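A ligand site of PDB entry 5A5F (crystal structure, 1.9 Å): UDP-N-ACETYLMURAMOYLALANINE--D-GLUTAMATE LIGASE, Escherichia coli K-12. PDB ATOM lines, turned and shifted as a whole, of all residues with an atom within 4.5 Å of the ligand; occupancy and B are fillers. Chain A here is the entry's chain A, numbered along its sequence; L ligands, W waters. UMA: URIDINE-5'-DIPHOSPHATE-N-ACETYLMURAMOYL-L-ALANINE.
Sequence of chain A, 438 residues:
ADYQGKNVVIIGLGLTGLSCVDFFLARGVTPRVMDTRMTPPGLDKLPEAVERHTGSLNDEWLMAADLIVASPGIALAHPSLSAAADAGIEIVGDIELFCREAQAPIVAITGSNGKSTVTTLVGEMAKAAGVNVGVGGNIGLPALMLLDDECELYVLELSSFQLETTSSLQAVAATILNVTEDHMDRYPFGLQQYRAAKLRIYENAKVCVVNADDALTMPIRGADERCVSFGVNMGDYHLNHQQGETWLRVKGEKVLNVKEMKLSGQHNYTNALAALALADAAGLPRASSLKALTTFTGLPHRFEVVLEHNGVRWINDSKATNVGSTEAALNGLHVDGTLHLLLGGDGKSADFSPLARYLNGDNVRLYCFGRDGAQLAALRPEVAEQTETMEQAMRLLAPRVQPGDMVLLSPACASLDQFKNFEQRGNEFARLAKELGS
An oxygen (O20) of the ligand sits at hydrogen-bond distance from the side-chain amide nitrogen (ND2) of Asn 138 (2.8 Å). N of Leu 15 lies within hydrogen-bond range of O1B of the ligand (3.1 Å). A ring nitrogen (NE2) of His 183 lies within hydrogen-bond range of an oxygen (O19) of the ligand (2.6 Å). The side-chain carboxylate (OD1) of Asp 35 sits at hydrogen-bond distance from a nitrogen (N3) of the ligand (3.4 Å). O2B of the ligand lies within hydrogen-bond range of N of Thr 16, 2.8 Å away. The backbone carbonyl oxygen (O) of Asn 138 is in hydrogen-bond range of an oxygen (O4') of the ligand, at 2.6 Å. The side-chain amide nitrogen of Gln 162 lies within hydrogen-bond range of an oxygen (O6') of the ligand, 3.0 Å away. An oxygen (O4B) of the ligand sits at hydrogen-bond distance from the guanidinium group (NH1) of Arg 37, at 2.9 Å. The side-chain hydroxyl of Thr 36 sits at hydrogen-bond distance from a nitrogen (N3) of the ligand. An oxygen (O4) of the ligand is in hydrogen-bond range of the backbone NH of Thr 36 (3.0 Å). OG1 of Thr 16 lies within hydrogen-bond range of O2B of the ligand (2.7 Å). O of Gly 137 sits at hydrogen-bond distance from O6' of the ligand (3.4 Å). N of Gly 73 sits at hydrogen-bond distance from O1A of the ligand (2.9 Å).
Merely in contact with the ligand: Ser 71, Gly 140, Pro 72, Ser 159, Gly 14, Phe 161 and Gly 12. Hydrophobic or aromatic side chains within 4 Å of the ligand: Leu 15, Pro 72, Phe 161 and His 183. Of the 24 residues printed, 17 come within 4 Å of the ligand. The nearest printed residue that does not touch the ligand is Ile 11 (4.03 Å).
Water W3 bridges O20 of the ligand and NZ of Lys 115. Water W1 lies within hydrogen-bond range of an oxygen (O6') of the ligand, the side-chain amide nitrogen (NE2) of Gln 162, the side-chain hydroxyl (OG1) of Thr 16 and the side-chain carboxylate (OD1) of Asp 94. Water W8 lies within hydrogen-bond range of OG of Ser 159 (2.7 Å), OD1 of Asn 138 (2.8 Å) and O7' of the ligand (2.8 Å). Water W6 bridges OD2 of Asp 94 (2.8 Å) and O6' of the ligand (2.9 Å). Water W2 lies within hydrogen-bond range of the side-chain hydroxyl of Ser 71, the backbone NH of Gly 14, an oxygen (O2A) of the ligand and the backbone carbonyl oxygen of Gly 12.
The side-chain carboxylate (OD2) of Asp 35 lies within salt-bridge range of the guanidinium group (NH2) of Arg 37 (2.7 Å). A ring nitrogen (NE2) of His 183 sits close to the side-chain carboxylate (OD2) of Asp 182, 3.4 Å away. The backbone NH (N) of Phe 161 sits close to the side-chain hydroxyl (OG) of Ser 159. The backbone NH (N) of Gln 162 lies within hydrogen-bond range of the side-chain hydroxyl (OG) of Ser 159. OG of Ser 71 sits at hydrogen-bond distance from O of Ile 11 (2.6 Å).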
ATOM      1  N   ILE A  11      19.337  12.797  22.830  1.00  0.00           N
ATOM      2  CA  ILE A  11      20.708  13.293  22.739  1.00  0.00           C
ATOM      3  C   ILE A  11      21.010  14.160  23.926  1.00  0.00           C
ATOM      4  O   ILE A  11      20.337  15.190  24.192  1.00  0.00           O
ATOM      5  CB  ILE A  11      20.976  14.095  21.445  1.00  0.00           C
ATOM      6  CG1 ILE A  11      20.775  13.237  20.199  1.00  0.00           C
ATOM      7  CG2 ILE A  11      22.378  14.691  21.455  1.00  0.00           C
ATOM      8  CD1 ILE A  11      20.659  14.058  18.921  1.00  0.00           C
ATOM      9  N   GLY A  12      22.062  13.776  24.630  1.00  0.00           N
ATOM     10  CA  GLY A  12      22.571  14.532  25.740  1.00  0.00           C
ATOM     11  C   GLY A  12      22.286  13.811  27.038  1.00  0.00           C
ATOM     12  O   GLY A  12      21.131  13.454  27.343  1.00  0.00           O
ATOM     13  N   GLY A  14      22.946  15.160  30.290  1.00  0.00           N
ATOM     14  CA  GLY A  14      22.935  16.003  31.491  1.00  0.00           C
ATOM     15  C   GLY A  14      21.568  15.938  32.205  1.00  0.00           C
ATOM     16  O   GLY A  14      20.855  14.917  32.087  1.00  0.00           O
ATOM     17  N   LEU A  15      21.189  17.026  32.906  1.00  0.00           N
ATOM     18  CA  LEU A  15      19.932  17.045  33.651  1.00  0.00           C
ATOM     19  C   LEU A  15      18.740  16.821  32.724  1.00  0.00           C
ATOM     20  O   LEU A  15      17.832  16.067  33.056  1.00  0.00           O
ATOM     21  CB  LEU A  15      19.733  18.341  34.412  1.00  0.00           C
ATOM     22  CG  LEU A  15      20.886  18.715  35.330  1.00  0.00           C
ATOM     23  CD1 LEU A  15      20.619  20.092  35.926  1.00  0.00           C
ATOM     24  CD2 LEU A  15      21.097  17.634  36.390  1.00  0.00           C
ATOM     25  N   THR A  16      18.794  17.444  31.570  1.00  0.00           N
ATOM     26  CA  THR A  16      17.694  17.348  30.621  1.00  0.00           C
ATOM     27  C   THR A  16      17.445  15.939  30.101  1.00  0.00           C
ATOM     28  O   THR A  16      16.309  15.433  30.196  1.00  0.00           O
ATOM     29  CB  THR A  16      17.858  18.322  29.459  1.00  0.00           C
ATOM     30  OG1 THR A  16      17.892  19.677  29.982  1.00  0.00           O
ATOM     31  CG2 THR A  16      16.676  18.174  28.458  1.00  0.00           C
ATOM     32  N   ASP A  35      25.435  10.628  23.679  1.00  0.00           N
ATOM     33  CA  ASP A  35      26.046  11.899  24.033  1.00  0.00           C
ATOM     34  C   ASP A  35      27.382  11.942  23.323  1.00  0.00           C
ATOM     35  O   ASP A  35      28.063  10.903  23.214  1.00  0.00           O
ATOM     36  CB  ASP A  35      26.222  11.960  25.559  1.00  0.00           C
ATOM     37  CG  ASP A  35      26.616  13.348  26.043  1.00  0.00           C
ATOM     38  OD1 ASP A  35      27.739  13.794  25.714  1.00  0.00           O
ATOM     39  OD2 ASP A  35      25.830  13.995  26.758  1.00  0.00           O
ATOM     40  N   THR A  36      27.789  13.126  22.847  1.00  0.00           N
ATOM     41  CA  THR A  36      29.075  13.239  22.128  1.00  0.00           C
ATOM     42  C   THR A  36      30.243  13.044  23.103  1.00  0.00           C
ATOM     43  O   THR A  36      31.359  12.759  22.692  1.00  0.00           O
ATOM     44  CB  THR A  36      29.249  14.610  21.402  1.00  0.00           C
ATOM     45  OG1 THR A  36      29.535  15.623  22.361  1.00  0.00           O
ATOM     46  CG2 THR A  36      28.006  15.015  20.647  1.00  0.00           C
ATOM     47  N   ARG A  37      30.014  13.241  24.388  1.00  0.00           N
ATOM     48  CA  ARG A  37      31.127  13.103  25.336  1.00  0.00           C
ATOM     49  C   ARG A  37      31.253  11.639  25.769  1.00  0.00           C
ATOM     50  O   ARG A  37      30.223  10.959  25.919  1.00  0.00           O
ATOM     51  CB  ARG A  37      30.928  13.993  26.559  1.00  0.00           C
ATOM     52  CG  ARG A  37      30.892  15.483  26.280  1.00  0.00           C
ATOM     53  CD  ARG A  37      30.217  16.228  27.424  1.00  0.00           C
ATOM     54  NE  ARG A  37      28.790  15.913  27.457  1.00  0.00           N
ATOM     55  CZ  ARG A  37      27.898  16.467  28.276  1.00  0.00           C
ATOM     56  NH1 ARG A  37      28.267  17.401  29.150  1.00  0.00           N
ATOM     57  NH2 ARG A  37      26.615  16.081  28.218  1.00  0.00           N
ATOM     58  N   SER A  71      18.570  17.580  23.863  1.00  0.00           N
ATOM     59  CA  SER A  71      18.965  18.500  24.937  1.00  0.00           C
ATOM     60  C   SER A  71      19.408  19.860  24.349  1.00  0.00           C
ATOM     61  O   SER A  71      19.902  19.900  23.198  1.00  0.00           O
ATOM     62  CB  SER A  71      20.122  17.884  25.757  1.00  0.00           C
ATOM     63  OG  SER A  71      19.719  16.627  26.318  1.00  0.00           O
ATOM     64  N   PRO A  72      19.192  20.965  25.104  1.00  0.00           N
ATOM     65  CA  PRO A  72      19.447  22.336  24.600  1.00  0.00           C
ATOM     66  C   PRO A  72      20.943  22.615  24.393  1.00  0.00           C
ATOM     67  O   PRO A  72      21.311  23.536  23.636  1.00  0.00           O
ATOM     68  CB  PRO A  72      18.920  23.245  25.747  1.00  0.00           C
ATOM     69  CG  PRO A  72      19.002  22.370  26.964  1.00  0.00           C
ATOM     70  CD  PRO A  72      18.671  20.965  26.495  1.00  0.00           C
ATOM     71  N   GLY A  73      21.768  21.817  25.040  1.00  0.00           N
ATOM     72  CA  GLY A  73      23.221  21.931  24.906  1.00  0.00           C
ATOM     73  C   GLY A  73      23.801  21.439  23.588  1.00  0.00           C
ATOM     74  O   GLY A  73      25.013  21.629  23.339  1.00  0.00           O
ATOM     75  N   ILE A  74      22.976  20.865  22.720  1.00  0.00           N
ATOM     76  CA  ILE A  74      23.460  20.519  21.352  1.00  0.00           C
ATOM     77  C   ILE A  74      22.687  21.279  20.273  1.00  0.00           C
ATOM     78  O   ILE A  74      21.453  21.393  20.343  1.00  0.00           O
ATOM     79  CB  ILE A  74      23.500  18.986  21.099  1.00  0.00           C
ATOM     80  CG1 ILE A  74      24.073  18.674  19.713  1.00  0.00           C
ATOM     81  CG2 ILE A  74      22.111  18.394  21.160  1.00  0.00           C
ATOM     82  CD1 ILE A  74      24.658  17.290  19.578  1.00  0.00           C
ATOM     83  N   ASP A  94      12.917  18.838  25.562  1.00  0.00           N
ATOM     84  CA  ASP A  94      12.129  18.557  26.758  1.00  0.00           C
ATOM     85  C   ASP A  94      10.985  19.525  26.959  1.00  0.00           C
ATOM     86  O   ASP A  94       9.916  19.133  27.464  1.00  0.00           O
ATOM     87  CB  ASP A  94      13.018  18.498  28.025  1.00  0.00           C
ATOM     88  CG  ASP A  94      13.601  19.855  28.436  1.00  0.00           C
ATOM     89  OD1 ASP A  94      14.163  20.612  27.596  1.00  0.00           O
ATOM     90  OD2 ASP A  94      13.610  20.153  29.671  1.00  0.00           O
ATOM     91  N   LYS A 115      16.328  36.495  33.989  1.00  0.00           N
ATOM     92  CA  LYS A 115      15.347  35.386  33.863  1.00  0.00           C
ATOM     93  C   LYS A 115      15.030  34.732  35.194  1.00  0.00           C
ATOM     94  O   LYS A 115      13.867  34.575  35.537  1.00  0.00           O
ATOM     95  CB  LYS A 115      15.808  34.308  32.884  1.00  0.00           C
ATOM     96  CG  LYS A 115      15.879  34.809  31.454  1.00  0.00           C
ATOM     97  CD  LYS A 115      16.372  33.747  30.480  1.00  0.00           C
ATOM     98  CE  LYS A 115      17.768  33.192  30.814  1.00  0.00           C
ATOM     99  NZ  LYS A 115      18.817  34.213  30.653  1.00  0.00           N
ATOM    100  N   GLY A 137      12.431  24.684  34.527  1.00  0.00           N
ATOM    101  CA  GLY A 137      13.016  25.012  33.216  1.00  0.00           C
ATOM    102  C   GLY A 137      14.476  25.372  33.358  1.00  0.00           C
ATOM    103  O   GLY A 137      15.193  24.822  34.206  1.00  0.00           O
ATOM    104  N   ASN A 138      14.926  26.316  32.542  1.00  0.00           N
ATOM    105  CA  ASN A 138      16.345  26.739  32.505  1.00  0.00           C
ATOM    106  C   ASN A 138      16.905  27.124  33.844  1.00  0.00           C
ATOM    107  O   ASN A 138      18.107  27.035  34.041  1.00  0.00           O
ATOM    108  CB  ASN A 138      16.525  27.958  31.557  1.00  0.00           C
ATOM    109  CG  ASN A 138      17.991  28.208  31.185  1.00  0.00           C
ATOM    110  OD1 ASN A 138      18.643  27.346  30.552  1.00  0.00           O
ATOM    111  ND2 ASN A 138      18.524  29.399  31.575  1.00  0.00           N
ATOM    112  N   ILE A 139      16.043  27.624  34.731  1.00  0.00           N
ATOM    113  CA  ILE A 139      16.413  28.025  36.087  1.00  0.00           C
ATOM    114  C   ILE A 139      17.169  26.885  36.799  1.00  0.00           C
ATOM    115  O   ILE A 139      17.970  27.131  37.698  1.00  0.00           O
ATOM    116  CB  ILE A 139      15.158  28.479  36.881  1.00  0.00           C
ATOM    117  CG1 ILE A 139      15.542  29.181  38.215  1.00  0.00           C
ATOM    118  CG2 ILE A 139      14.170  27.306  37.070  1.00  0.00           C
ATOM    119  CD1 ILE A 139      14.360  29.969  38.738  1.00  0.00           C
ATOM    120  N   GLY A 140      16.865  25.650  36.452  1.00  0.00           N
ATOM    121  CA  GLY A 140      17.705  24.551  36.893  1.00  0.00           C
ATOM    122  C   GLY A 140      16.951  23.296  37.312  1.00  0.00           C
ATOM    123  O   GLY A 140      17.560  22.289  37.646  1.00  0.00           O
ATOM    124  N   PRO A 142      14.649  20.645  35.714  1.00  0.00           N
ATOM    125  CA  PRO A 142      14.103  20.299  34.385  1.00  0.00           C
ATOM    126  C   PRO A 142      12.548  20.247  34.395  1.00  0.00           C
ATOM    127  O   PRO A 142      11.943  19.703  35.299  1.00  0.00           O
ATOM    128  CB  PRO A 142      14.711  18.906  34.099  1.00  0.00           C
ATOM    129  CG  PRO A 142      15.930  18.847  34.947  1.00  0.00           C
ATOM    130  CD  PRO A 142      15.621  19.646  36.193  1.00  0.00           C
ATOM    131  N   SER A 159      15.445  29.196  27.745  1.00  0.00           N
ATOM    132  CA  SER A 159      16.635  29.701  26.993  1.00  0.00           C
ATOM    133  C   SER A 159      16.233  29.760  25.553  1.00  0.00           C
ATOM    134  O   SER A 159      15.315  29.049  25.148  1.00  0.00           O
ATOM    135  CB  SER A 159      17.834  28.726  27.096  1.00  0.00           C
ATOM    136  OG  SER A 159      17.493  27.474  26.486  1.00  0.00           O
ATOM    137  N   PHE A 161      17.973  28.260  23.395  1.00  0.00           N
ATOM    138  CA  PHE A 161      18.255  26.896  22.933  1.00  0.00           C
ATOM    139  C   PHE A 161      16.963  26.076  23.065  1.00  0.00           C
ATOM    140  O   PHE A 161      16.584  25.347  22.161  1.00  0.00           O
ATOM    141  CB  PHE A 161      19.332  26.239  23.823  1.00  0.00           C
ATOM    142  CG  PHE A 161      20.690  26.919  23.797  1.00  0.00           C
ATOM    143  CD1 PHE A 161      21.106  27.684  22.715  1.00  0.00           C
ATOM    144  CD2 PHE A 161      21.588  26.720  24.860  1.00  0.00           C
ATOM    145  CE1 PHE A 161      22.363  28.287  22.706  1.00  0.00           C
ATOM    146  CE2 PHE A 161      22.855  27.309  24.853  1.00  0.00           C
ATOM    147  CZ  PHE A 161      23.242  28.088  23.773  1.00  0.00           C
ATOM    148  N   GLN A 162      16.345  26.144  24.242  1.00  0.00           N
ATOM    149  CA  GLN A 162      15.093  25.373  24.480  1.00  0.00           C
ATOM    150  C   GLN A 162      13.982  25.856  23.538  1.00  0.00           C
ATOM    151  O   GLN A 162      13.255  25.048  22.973  1.00  0.00           O
ATOM    152  CB  GLN A 162      14.631  25.560  25.938  1.00  0.00           C
ATOM    153  CG  GLN A 162      15.523  24.840  26.938  1.00  0.00           C
ATOM    154  CD  GLN A 162      15.258  25.294  28.371  1.00  0.00           C
ATOM    155  OE1 GLN A 162      14.931  26.449  28.621  1.00  0.00           O
ATOM    156  NE2 GLN A 162      15.401  24.371  29.313  1.00  0.00           N
ATOM    157  N   ASP A 182      24.649  37.219  23.569  1.00  0.00           N
ATOM    158  CA  ASP A 182      25.050  36.054  24.348  1.00  0.00           C
ATOM    159  C   ASP A 182      24.994  34.724  23.585  1.00  0.00           C
ATOM    160  O   ASP A 182      24.182  34.547  22.670  1.00  0.00           O
ATOM    161  CB  ASP A 182      24.258  35.936  25.665  1.00  0.00           C
ATOM    162  CG  ASP A 182      24.873  34.929  26.645  1.00  0.00           C
ATOM    163  OD1 ASP A 182      26.124  34.850  26.712  1.00  0.00           O
ATOM    164  OD2 ASP A 182      24.120  34.200  27.320  1.00  0.00           O
ATOM    165  N   HIS A 183      25.846  33.782  24.012  1.00  0.00           N
ATOM    166  CA  HIS A 183      25.949  32.449  23.398  1.00  0.00           C
ATOM    167  C   HIS A 183      26.240  32.514  21.907  1.00  0.00           C
ATOM    168  O   HIS A 183      25.759  31.677  21.132  1.00  0.00           O
ATOM    169  CB  HIS A 183      24.682  31.628  23.667  1.00  0.00           C
ATOM    170  CG  HIS A 183      24.531  31.198  25.093  1.00  0.00           C
ATOM    171  ND1 HIS A 183      25.468  30.423  25.736  1.00  0.00           N
ATOM    172  CD2 HIS A 183      23.553  31.437  25.996  1.00  0.00           C
ATOM    173  CE1 HIS A 183      25.077  30.212  26.979  1.00  0.00           C
ATOM    174  NE2 HIS A 183      23.908  30.810  27.163  1.00  0.00           N
HETATM  175  N1  UMA L   1      26.964  18.434  25.604  1.00  0.00           N
HETATM  176  C2  UMA L   1      27.909  17.736  24.820  1.00  0.00           C
HETATM  177  N3  UMA L   1      27.525  16.698  24.050  1.00  0.00           N
HETATM  178  C4  UMA L   1      26.241  16.330  24.040  1.00  0.00           C
HETATM  179  C5  UMA L   1      25.274  16.998  24.821  1.00  0.00           C
HETATM  180  C6  UMA L   1      25.673  18.057  25.613  1.00  0.00           C
HETATM  181  O2  UMA L   1      29.095  18.093  24.852  1.00  0.00           O
HETATM  182  O4  UMA L   1      25.888  15.378  23.316  1.00  0.00           O
HETATM  183  C1B UMA L   1      27.456  19.517  26.454  1.00  0.00           C
HETATM  184  C2B UMA L   1      27.256  20.900  25.854  1.00  0.00           C
HETATM  185  O2' UMA L   1      28.548  21.481  25.815  1.00  0.00           O
HETATM  186  C3B UMA L   1      26.516  21.693  26.909  1.00  0.00           C
HETATM  187  C4B UMA L   1      26.577  20.839  28.176  1.00  0.00           C
HETATM  188  O4B UMA L   1      26.847  19.486  27.758  1.00  0.00           O
HETATM  189  O3B UMA L   1      27.255  22.877  27.143  1.00  0.00           O
HETATM  190  C5B UMA L   1      25.248  20.883  28.914  1.00  0.00           C
HETATM  191  O5B UMA L   1      24.212  20.701  27.939  1.00  0.00           O
HETATM  192  PA  UMA L   1      22.900  19.846  28.359  1.00  0.00           P
HETATM  193  O1A UMA L   1      21.808  20.104  27.339  1.00  0.00           O
HETATM  194  O2A UMA L   1      23.330  18.427  28.664  1.00  0.00           O
HETATM  195  O3A UMA L   1      22.599  20.629  29.712  1.00  0.00           O
HETATM  196  PB  UMA L   1      21.679  20.163  30.937  1.00  0.00           P
HETATM  197  O1B UMA L   1      22.586  19.660  32.041  1.00  0.00           O
HETATM  198  O2B UMA L   1      20.498  19.365  30.499  1.00  0.00           O
HETATM  199  O1' UMA L   1      21.218  21.628  31.406  1.00  0.00           O
HETATM  200  C1' UMA L   1      20.261  22.333  30.607  1.00  0.00           C
HETATM  201  C2' UMA L   1      20.632  23.802  30.613  1.00  0.00           C
HETATM  202  N2' UMA L   1      21.959  23.888  30.012  1.00  0.00           N
HETATM  203  C7' UMA L   1      22.160  24.451  28.787  1.00  0.00           C
HETATM  204  O7' UMA L   1      21.250  24.660  27.990  1.00  0.00           O
HETATM  205  C8' UMA L   1      23.564  24.867  28.442  1.00  0.00           C
HETATM  206  C3' UMA L   1      20.562  24.346  32.044  1.00  0.00           C
HETATM  207  O3' UMA L   1      20.814  25.741  32.025  1.00  0.00           O
HETATM  208  C4' UMA L   1      19.150  24.136  32.537  1.00  0.00           C
HETATM  209  O4' UMA L   1      19.094  24.595  33.891  1.00  0.00           O
HETATM  210  C5' UMA L   1      18.768  22.631  32.476  1.00  0.00           C
HETATM  211  O5' UMA L   1      18.972  22.105  31.163  1.00  0.00           O
HETATM  212  C6' UMA L   1      17.293  22.380  32.791  1.00  0.00           C
HETATM  213  O6' UMA L   1      16.435  22.896  31.733  1.00  0.00           O
HETATM  214  C18 UMA L   1      22.142  26.134  32.444  1.00  0.00           C
HETATM  215  C19 UMA L   1      22.635  27.103  31.413  1.00  0.00           C
HETATM  216  O18 UMA L   1      23.806  27.439  31.364  1.00  0.00           O
HETATM  217  C20 UMA L   1      22.087  26.811  33.823  1.00  0.00           C
HETATM  218  N4  UMA L   1      21.738  27.564  30.541  1.00  0.00           N
HETATM  219  C21 UMA L   1      22.090  28.525  29.517  1.00  0.00           C
HETATM  220  C22 UMA L   1      21.904  29.960  29.994  1.00  0.00           C
HETATM  221  O19 UMA L   1      22.557  30.863  29.404  1.00  0.00           O
HETATM  222  O20 UMA L   1      21.111  30.232  30.957  1.00  0.00           O
HETATM  223  C23 UMA L   1      21.209  28.231  28.297  1.00  0.00           C
HETATM  224  O   HOH W   1      16.266  21.789  29.298  1.00  0.00           O
HETATM  225  O   HOH W   2      20.938  16.634  28.724  1.00  0.00           O
HETATM  226  O   HOH W   3      20.798  32.404  32.402  1.00  0.00           O
HETATM  227  O   HOH W   4      23.304  21.805  34.019  1.00  0.00           O
HETATM  228  O   HOH W   5      24.961  18.537  32.487  1.00  0.00           O
HETATM  229  O   HOH W   6      13.639  22.171  31.627  1.00  0.00           O
HETATM  230  O   HOH W   7      24.292  23.375  31.466  1.00  0.00           O
HETATM  231  O   HOH W   8      18.672  25.767  28.284  1.00  0.00           O
